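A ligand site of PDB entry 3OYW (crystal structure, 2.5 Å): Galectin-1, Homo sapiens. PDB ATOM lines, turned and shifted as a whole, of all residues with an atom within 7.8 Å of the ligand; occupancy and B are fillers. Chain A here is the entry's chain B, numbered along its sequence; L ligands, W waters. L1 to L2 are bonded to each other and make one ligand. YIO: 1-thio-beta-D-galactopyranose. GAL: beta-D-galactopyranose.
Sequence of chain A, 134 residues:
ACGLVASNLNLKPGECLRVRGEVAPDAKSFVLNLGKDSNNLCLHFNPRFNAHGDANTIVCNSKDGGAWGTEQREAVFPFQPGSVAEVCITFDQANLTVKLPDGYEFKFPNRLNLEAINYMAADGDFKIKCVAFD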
ATOM      1  N   SER A  29      24.931 -24.904  -7.816  1.00  0.00           N
ATOM      2  CA  SER A  29      24.308 -24.356  -9.023  1.00  0.00           C
ATOM      3  C   SER A  29      25.140 -23.203  -9.561  1.00  0.00           C
ATOM      4  O   SER A  29      25.860 -22.550  -8.813  1.00  0.00           O
ATOM      5  CB  SER A  29      22.889 -23.863  -8.740  1.00  0.00           C
ATOM      6  OG  SER A  29      22.905 -22.491  -8.381  1.00  0.00           O
ATOM      7  N   PHE A  30      25.012 -22.952 -10.865  1.00  0.00           N
ATOM      8  CA  PHE A  30      25.479 -21.688 -11.435  1.00  0.00           C
ATOM      9  C   PHE A  30      24.506 -21.074 -12.434  1.00  0.00           C
ATOM     10  O   PHE A  30      23.547 -21.710 -12.864  1.00  0.00           O
ATOM     11  CB  PHE A  30      26.904 -21.784 -11.971  1.00  0.00           C
ATOM     12  CG  PHE A  30      27.045 -22.601 -13.233  1.00  0.00           C
ATOM     13  CD1 PHE A  30      27.133 -21.975 -14.481  1.00  0.00           C
ATOM     14  CD2 PHE A  30      27.139 -23.992 -13.178  1.00  0.00           C
ATOM     15  CE1 PHE A  30      27.292 -22.710 -15.648  1.00  0.00           C
ATOM     16  CE2 PHE A  30      27.283 -24.740 -14.344  1.00  0.00           C
ATOM     17  CZ  PHE A  30      27.367 -24.093 -15.580  1.00  0.00           C
ATOM     18  N   VAL A  31      24.755 -19.809 -12.774  1.00  0.00           N
ATOM     19  CA  VAL A  31      23.826 -19.026 -13.564  1.00  0.00           C
ATOM     20  C   VAL A  31      24.559 -18.259 -14.662  1.00  0.00           C
ATOM     21  O   VAL A  31      25.548 -17.579 -14.401  1.00  0.00           O
ATOM     22  CB  VAL A  31      23.038 -18.050 -12.665  1.00  0.00           C
ATOM     23  CG1 VAL A  31      22.375 -16.944 -13.473  1.00  0.00           C
ATOM     24  CG2 VAL A  31      21.994 -18.825 -11.857  1.00  0.00           C
ATOM     25  N   ASN A  33      23.224 -15.414 -17.333  1.00  0.00           N
ATOM     26  CA  ASN A  33      22.101 -14.566 -17.744  1.00  0.00           C
ATOM     27  C   ASN A  33      22.437 -13.770 -18.994  1.00  0.00           C
ATOM     28  O   ASN A  33      23.482 -13.124 -19.065  1.00  0.00           O
ATOM     29  CB  ASN A  33      21.748 -13.568 -16.647  1.00  0.00           C
ATOM     30  CG  ASN A  33      20.999 -14.185 -15.507  1.00  0.00           C
ATOM     31  OD1 ASN A  33      20.437 -15.280 -15.628  1.00  0.00           O
ATOM     32  ND2 ASN A  33      20.969 -13.483 -14.377  1.00  0.00           N
ATOM     33  N   HIS A  44      17.918 -17.089 -19.019  1.00  0.00           N
ATOM     34  CA  HIS A  44      18.448 -17.404 -17.705  1.00  0.00           C
ATOM     35  C   HIS A  44      18.819 -18.889 -17.743  1.00  0.00           C
ATOM     36  O   HIS A  44      17.953 -19.751 -17.818  1.00  0.00           O
ATOM     37  CB  HIS A  44      17.383 -17.119 -16.638  1.00  0.00           C
ATOM     38  CG  HIS A  44      17.710 -17.658 -15.284  1.00  0.00           C
ATOM     39  ND1 HIS A  44      18.571 -17.024 -14.417  1.00  0.00           N
ATOM     40  CD2 HIS A  44      17.268 -18.771 -14.637  1.00  0.00           C
ATOM     41  CE1 HIS A  44      18.663 -17.722 -13.300  1.00  0.00           C
ATOM     42  NE2 HIS A  44      17.886 -18.791 -13.417  1.00  0.00           N
ATOM     43  N   PHE A  45      20.117 -19.178 -17.732  1.00  0.00           N
ATOM     44  CA  PHE A  45      20.636 -20.539 -17.906  1.00  0.00           C
ATOM     45  C   PHE A  45      21.148 -21.035 -16.551  1.00  0.00           C
ATOM     46  O   PHE A  45      22.136 -20.505 -16.031  1.00  0.00           O
ATOM     47  CB  PHE A  45      21.761 -20.484 -18.947  1.00  0.00           C
ATOM     48  CG  PHE A  45      22.490 -21.773 -19.170  1.00  0.00           C
ATOM     49  CD1 PHE A  45      21.889 -22.835 -19.839  1.00  0.00           C
ATOM     50  CD2 PHE A  45      23.809 -21.911 -18.756  1.00  0.00           C
ATOM     51  CE1 PHE A  45      22.589 -24.026 -20.080  1.00  0.00           C
ATOM     52  CE2 PHE A  45      24.520 -23.100 -18.984  1.00  0.00           C
ATOM     53  CZ  PHE A  45      23.903 -24.157 -19.648  1.00  0.00           C
ATOM     54  N   ASN A  46      20.490 -22.033 -15.984  1.00  0.00           N
ATOM     55  CA  ASN A  46      20.744 -22.397 -14.571  1.00  0.00           C
ATOM     56  C   ASN A  46      20.903 -23.914 -14.305  1.00  0.00           C
ATOM     57  O   ASN A  46      19.964 -24.579 -13.856  1.00  0.00           O
ATOM     58  CB  ASN A  46      19.646 -21.786 -13.680  1.00  0.00           C
ATOM     59  CG  ASN A  46      19.814 -22.104 -12.199  1.00  0.00           C
ATOM     60  OD1 ASN A  46      18.824 -22.096 -11.451  1.00  0.00           O
ATOM     61  ND2 ASN A  46      21.038 -22.377 -11.753  1.00  0.00           N
ATOM     62  N   ARG A  48      21.506 -26.914 -12.278  1.00  0.00           N
ATOM     63  CA  ARG A  48      21.396 -27.230 -10.857  1.00  0.00           C
ATOM     64  C   ARG A  48      21.968 -28.616 -10.574  1.00  0.00           C
ATOM     65  O   ARG A  48      21.361 -29.644 -10.930  1.00  0.00           O
ATOM     66  CB  ARG A  48      19.943 -27.107 -10.398  1.00  0.00           C
ATOM     67  CG  ARG A  48      19.385 -25.713 -10.579  1.00  0.00           C
ATOM     68  CD  ARG A  48      17.921 -25.584 -10.205  1.00  0.00           C
ATOM     69  NE  ARG A  48      17.447 -24.240 -10.520  1.00  0.00           N
ATOM     70  CZ  ARG A  48      16.195 -23.805 -10.378  1.00  0.00           C
ATOM     71  NH1 ARG A  48      15.886 -22.570 -10.710  1.00  0.00           N
ATOM     72  NH2 ARG A  48      15.253 -24.622  -9.908  1.00  0.00           N
ATOM     73  N   ALA A  51      20.134 -28.092  -5.999  1.00  0.00           N
ATOM     74  CA  ALA A  51      19.586 -26.800  -5.566  1.00  0.00           C
ATOM     75  C   ALA A  51      18.082 -26.757  -5.845  1.00  0.00           C
ATOM     76  O   ALA A  51      17.622 -27.307  -6.857  1.00  0.00           O
ATOM     77  CB  ALA A  51      20.286 -25.644  -6.280  1.00  0.00           C
ATOM     78  N   HIS A  52      17.338 -26.103  -4.948  1.00  0.00           N
ATOM     79  CA  HIS A  52      15.884 -25.962  -5.041  1.00  0.00           C
ATOM     80  C   HIS A  52      15.134 -27.305  -5.198  1.00  0.00           C
ATOM     81  O   HIS A  52      14.009 -27.334  -5.708  1.00  0.00           O
ATOM     82  CB  HIS A  52      15.485 -25.002  -6.172  1.00  0.00           C
ATOM     83  CG  HIS A  52      16.019 -23.616  -6.006  1.00  0.00           C
ATOM     84  ND1 HIS A  52      17.196 -23.206  -6.579  1.00  0.00           N
ATOM     85  CD2 HIS A  52      15.537 -22.558  -5.326  1.00  0.00           C
ATOM     86  CE1 HIS A  52      17.424 -21.940  -6.269  1.00  0.00           C
ATOM     87  NE2 HIS A  52      16.425 -21.523  -5.501  1.00  0.00           N
ATOM     88  N   GLY A  53      15.755 -28.391  -4.761  1.00  0.00           N
ATOM     89  CA  GLY A  53      15.152 -29.723  -4.914  1.00  0.00           C
ATOM     90  C   GLY A  53      15.342 -30.324  -6.291  1.00  0.00           C
ATOM     91  O   GLY A  53      14.758 -31.361  -6.603  1.00  0.00           O
ATOM     92  N   ASP A  54      16.157 -29.667  -7.113  1.00  0.00           N
ATOM     93  CA  ASP A  54      16.574 -30.206  -8.405  1.00  0.00           C
ATOM     94  C   ASP A  54      17.972 -30.798  -8.288  1.00  0.00           C
ATOM     95  O   ASP A  54      18.866 -30.181  -7.699  1.00  0.00           O
ATOM     96  CB  ASP A  54      16.591 -29.101  -9.479  1.00  0.00           C
ATOM     97  CG  ASP A  54      15.212 -28.563  -9.782  1.00  0.00           C
ATOM     98  OD1 ASP A  54      14.276 -29.365  -9.984  1.00  0.00           O
ATOM     99  OD2 ASP A  54      15.058 -27.319  -9.823  1.00  0.00           O
ATOM    100  N   VAL A  59      17.869 -25.811 -15.702  1.00  0.00           N
ATOM    101  CA  VAL A  59      16.636 -25.064 -15.715  1.00  0.00           C
ATOM    102  C   VAL A  59      16.868 -23.822 -16.560  1.00  0.00           C
ATOM    103  O   VAL A  59      17.851 -23.091 -16.346  1.00  0.00           O
ATOM    104  CB  VAL A  59      16.206 -24.670 -14.272  1.00  0.00           C
ATOM    105  CG1 VAL A  59      15.013 -23.734 -14.278  1.00  0.00           C
ATOM    106  CG2 VAL A  59      15.929 -25.920 -13.426  1.00  0.00           C
ATOM    107  N   CYS A  60      15.970 -23.596 -17.523  1.00  0.00           N
ATOM    108  CA  CYS A  60      15.977 -22.394 -18.360  1.00  0.00           C
ATOM    109  C   CYS A  60      14.673 -21.597 -18.234  1.00  0.00           C
ATOM    110  O   CYS A  60      13.576 -22.147 -18.154  1.00  0.00           O
ATOM    111  CB  CYS A  60      16.195 -22.754 -19.834  1.00  0.00           C
ATOM    112  SG  CYS A  60      17.816 -23.437 -20.189  1.00  0.00           S
ATOM    113  N   ASN A  61      14.809 -20.276 -18.225  1.00  0.00           N
ATOM    114  CA  ASN A  61      13.663 -19.374 -18.145  1.00  0.00           C
ATOM    115  C   ASN A  61      14.015 -18.058 -18.818  1.00  0.00           C
ATOM    116  O   ASN A  61      15.165 -17.854 -19.227  1.00  0.00           O
ATOM    117  CB  ASN A  61      13.252 -19.143 -16.681  1.00  0.00           C
ATOM    118  CG  ASN A  61      11.782 -18.789 -16.533  1.00  0.00           C
ATOM    119  OD1 ASN A  61      11.114 -18.467 -17.517  1.00  0.00           O
ATOM    120  ND2 ASN A  61      11.272 -18.853 -15.306  1.00  0.00           N
ATOM    121  N   SER A  62      13.016 -17.179 -18.934  1.00  0.00           N
ATOM    122  CA  SER A  62      13.211 -15.794 -19.377  1.00  0.00           C
ATOM    123  C   SER A  62      12.714 -14.858 -18.295  1.00  0.00           C
ATOM    124  O   SER A  62      12.111 -15.271 -17.304  1.00  0.00           O
ATOM    125  CB  SER A  62      12.425 -15.526 -20.654  1.00  0.00           C
ATOM    126  OG  SER A  62      11.075 -15.916 -20.459  1.00  0.00           O
ATOM    127  N   TRP A  68       9.516 -13.272 -14.149  1.00  0.00           N
ATOM    128  CA  TRP A  68       9.964 -14.573 -14.642  1.00  0.00           C
ATOM    129  C   TRP A  68       8.914 -15.200 -15.544  1.00  0.00           C
ATOM    130  O   TRP A  68       7.722 -15.156 -15.222  1.00  0.00           O
ATOM    131  CB  TRP A  68      10.211 -15.535 -13.475  1.00  0.00           C
ATOM    132  CG  TRP A  68      11.468 -15.280 -12.676  1.00  0.00           C
ATOM    133  CD1 TRP A  68      11.536 -14.921 -11.366  1.00  0.00           C
ATOM    134  CD2 TRP A  68      12.823 -15.408 -13.128  1.00  0.00           C
ATOM    135  NE1 TRP A  68      12.852 -14.802 -10.964  1.00  0.00           N
ATOM    136  CE2 TRP A  68      13.660 -15.090 -12.038  1.00  0.00           C
ATOM    137  CE3 TRP A  68      13.411 -15.742 -14.359  1.00  0.00           C
ATOM    138  CZ2 TRP A  68      15.049 -15.104 -12.134  1.00  0.00           C
ATOM    139  CZ3 TRP A  68      14.792 -15.745 -14.450  1.00  0.00           C
ATOM    140  CH2 TRP A  68      15.603 -15.425 -13.347  1.00  0.00           C
ATOM    141  N   GLY A  69       9.358 -15.804 -16.641  1.00  0.00           N
ATOM    142  CA  GLY A  69       8.450 -16.584 -17.490  1.00  0.00           C
ATOM    143  C   GLY A  69       8.308 -18.011 -16.957  1.00  0.00           C
ATOM    144  O   GLY A  69       8.617 -18.273 -15.787  1.00  0.00           O
ATOM    145  N   THR A  70       7.849 -18.914 -17.812  1.00  0.00           N
ATOM    146  CA  THR A  70       7.705 -20.336 -17.462  1.00  0.00           C
ATOM    147  C   THR A  70       9.014 -21.113 -17.629  1.00  0.00           C
ATOM    148  O   THR A  70       9.724 -20.975 -18.636  1.00  0.00           O
ATOM    149  CB  THR A  70       6.617 -21.009 -18.321  1.00  0.00           C
ATOM    150  OG1 THR A  70       5.431 -20.223 -18.315  1.00  0.00           O
ATOM    151  CG2 THR A  70       6.297 -22.391 -17.780  1.00  0.00           C
ATOM    152  N   GLU A  71       9.322 -21.960 -16.653  1.00  0.00           N
ATOM    153  CA  GLU A  71      10.541 -22.772 -16.672  1.00  0.00           C
ATOM    154  C   GLU A  71      10.500 -23.900 -17.702  1.00  0.00           C
ATOM    155  O   GLU A  71       9.475 -24.588 -17.845  1.00  0.00           O
ATOM    156  CB  GLU A  71      10.807 -23.376 -15.296  1.00  0.00           C
ATOM    157  CG  GLU A  71      11.452 -22.421 -14.319  1.00  0.00           C
ATOM    158  CD  GLU A  71      11.668 -23.044 -12.949  1.00  0.00           C
ATOM    159  OE1 GLU A  71      11.337 -24.235 -12.745  1.00  0.00           O
ATOM    160  OE2 GLU A  71      12.192 -22.328 -12.059  1.00  0.00           O
ATOM    161  N   GLN A  72      11.615 -24.104 -18.395  1.00  0.00           N
ATOM    162  CA  GLN A  72      11.833 -25.307 -19.190  1.00  0.00           C
ATOM    163  C   GLN A  72      12.976 -26.100 -18.595  1.00  0.00           C
ATOM    164  O   GLN A  72      14.004 -25.552 -18.207  1.00  0.00           O
ATOM    165  CB  GLN A  72      12.132 -24.958 -20.650  1.00  0.00           C
ATOM    166  CG  GLN A  72      12.003 -26.144 -21.589  1.00  0.00           C
ATOM    167  CD  GLN A  72      12.213 -25.765 -23.043  1.00  0.00           C
ATOM    168  OE1 GLN A  72      13.340 -25.536 -23.494  1.00  0.00           O
ATOM    169  NE2 GLN A  72      11.124 -25.683 -23.784  1.00  0.00           N
ATOM    170  N   ARG A  73      12.772 -27.411 -18.527  1.00  0.00           N
ATOM    171  CA  ARG A  73      13.785 -28.317 -17.975  1.00  0.00           C
ATOM    172  C   ARG A  73      14.402 -29.150 -19.079  1.00  0.00           C
ATOM    173  O   ARG A  73      13.691 -29.829 -19.813  1.00  0.00           O
ATOM    174  CB  ARG A  73      13.161 -29.204 -16.905  1.00  0.00           C
ATOM    175  CG  ARG A  73      13.152 -28.542 -15.559  1.00  0.00           C
ATOM    176  CD  ARG A  73      11.798 -28.586 -14.883  1.00  0.00           C
ATOM    177  NE  ARG A  73      11.743 -27.589 -13.813  1.00  0.00           N
ATOM    178  CZ  ARG A  73      12.320 -27.735 -12.616  1.00  0.00           C
ATOM    179  NH1 ARG A  73      12.232 -26.775 -11.708  1.00  0.00           N
ATOM    180  NH2 ARG A  73      13.005 -28.849 -12.341  1.00  0.00           N
ATOM    181  N   ASP A 123      26.711 -15.902 -12.154  1.00  0.00           N
ATOM    182  CA  ASP A 123      26.477 -15.984 -10.714  1.00  0.00           C
ATOM    183  C   ASP A 123      26.604 -17.428 -10.241  1.00  0.00           C
ATOM    184  O   ASP A 123      26.497 -18.360 -11.037  1.00  0.00           O
ATOM    185  CB  ASP A 123      25.086 -15.425 -10.373  1.00  0.00           C
ATOM    186  CG  ASP A 123      24.957 -14.987  -8.918  1.00  0.00           C
ATOM    187  OD1 ASP A 123      25.977 -14.922  -8.183  1.00  0.00           O
ATOM    188  OD2 ASP A 123      23.816 -14.695  -8.498  1.00  0.00           O
HETATM  189  C1  YIO L   1      13.801 -19.891  -8.975  1.00  0.00           C
HETATM  190  C2  YIO L   1      15.159 -19.378  -8.533  1.00  0.00           C
HETATM  191  C3  YIO L   1      15.659 -18.248  -9.442  1.00  0.00           C
HETATM  192  C4  YIO L   1      15.584 -18.675 -10.905  1.00  0.00           C
HETATM  193  C5  YIO L   1      14.166 -19.107 -11.265  1.00  0.00           C
HETATM  194  C6  YIO L   1      14.131 -19.582 -12.718  1.00  0.00           C
HETATM  195  O2  YIO L   1      15.098 -18.967  -7.159  1.00  0.00           O
HETATM  196  O3  YIO L   1      17.022 -17.960  -9.158  1.00  0.00           O
HETATM  197  O4  YIO L   1      16.485 -19.765 -11.143  1.00  0.00           O
HETATM  198  O5  YIO L   1      13.723 -20.169 -10.392  1.00  0.00           O
HETATM  199  O6  YIO L   1      12.796 -19.941 -13.075  1.00  0.00           O
HETATM  200  S1  YIO L   1      13.518 -21.381  -8.058  1.00  0.00           S
HETATM  201  C1  GAL L   2      11.896 -21.665  -8.680  1.00  0.00           C
HETATM  202  C2  GAL L   2      11.660 -23.166  -8.889  1.00  0.00           C
HETATM  203  C3  GAL L   2      10.238 -23.369  -9.408  1.00  0.00           C
HETATM  204  C4  GAL L   2       9.234 -22.726  -8.459  1.00  0.00           C
HETATM  205  C5  GAL L   2       9.558 -21.239  -8.253  1.00  0.00           C
HETATM  206  C6  GAL L   2       8.592 -20.591  -7.260  1.00  0.00           C
HETATM  207  O2  GAL L   2      12.586 -23.713  -9.836  1.00  0.00           O
HETATM  208  O3  GAL L   2       9.986 -24.767  -9.576  1.00  0.00           O
HETATM  209  O4  GAL L   2       9.246 -23.409  -7.202  1.00  0.00           O
HETATM  210  O5  GAL L   2      10.917 -21.089  -7.796  1.00  0.00           O
HETATM  211  O6  GAL L   2       8.711 -19.159  -7.305  1.00  0.00           O
HETATM  212  O   HOH W   1      19.151 -19.780  -9.630  1.00  0.00           O
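An oxygen (O2) of GAL L2 is in hydrogen-bond range of the side-chain carboxylate (OE2) of Glu 71, 2.6 Å away.
NH2 of Arg 48 lies within hydrogen-bond range of O2 of GAL L2 (2.8 Å).
An oxygen (O4) of YIO L1 lies within hydrogen-bond range of a ring nitrogen (NE2) of His 44 (2.8 Å).
The side-chain amide nitrogen (ND2) of Asn 61 lies within hydrogen-bond range of an oxygen (O6) of YIO L1 (2.9 Å).
An oxygen (O4) of YIO L1 is in hydrogen-bond range of the side-chain amide oxygen (OD1) of Asn 46, 3.3 Å away.
NE2 of His 52 sits at hydrogen-bond distance from O2 of YIO L1 (3.3 Å).
The side-chain carboxylate (OE1) of Glu 71 is in salt-bridge range of the guanidinium group (NH1) of Arg 73.
The guanidinium group (NH2) of Arg 48 is in salt-bridge range of the side-chain carboxylate (OD2) of Asp 54 (2.7 Å).
The backbone NH (N) of His 44 is in hydrogen-bond range of the backbone carbonyl oxygen (O) of Asn 61.
A ring nitrogen (ND1) of His 44 lies within hydrogen-bond range of the side-chain amide oxygen (OD1) of Asn 33, at 2.8 Å.
The backbone carbonyl oxygen of Gly 69 is in hydrogen-bond range of the side-chain amide nitrogen of Asn 61 (2.8 Å).
The side-chain amide oxygen (OD1) of Asn 61 sits close to the backbone carbonyl oxygen (O) of Thr 70 (3.1 Å).
The backbone NH (N) of Asn 46 is in hydrogen-bond range of the backbone carbonyl oxygen (O) of Val 59 (2.9 Å).
The guanidinium group (NH2) of Arg 73 lies within salt-bridge range of the side-chain carboxylate (OD1) of Asp 54.
Merely in contact with the ligand: Trp 68 and Arg 73.
Hydrophobic or aromatic side chains that line the ligand: His 44, His 52 and Trp 68.
Eight residues have an atom within 4 Å of the ligand: His 44, Asn 46, Arg 48, His 52, Asn 61, Trp 68, Glu 71 and Arg 73.
Along chain A the residues within 4 Å of the ligand span positions 44 to 73.
The nearest printed residue that does not touch the ligand is Asp 54 (4.4 Å).
Water W1 lies within hydrogen-bond range of O3 of YIO L1 (2.8 Å) and OD1 of Asn 46 (3.0 Å).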
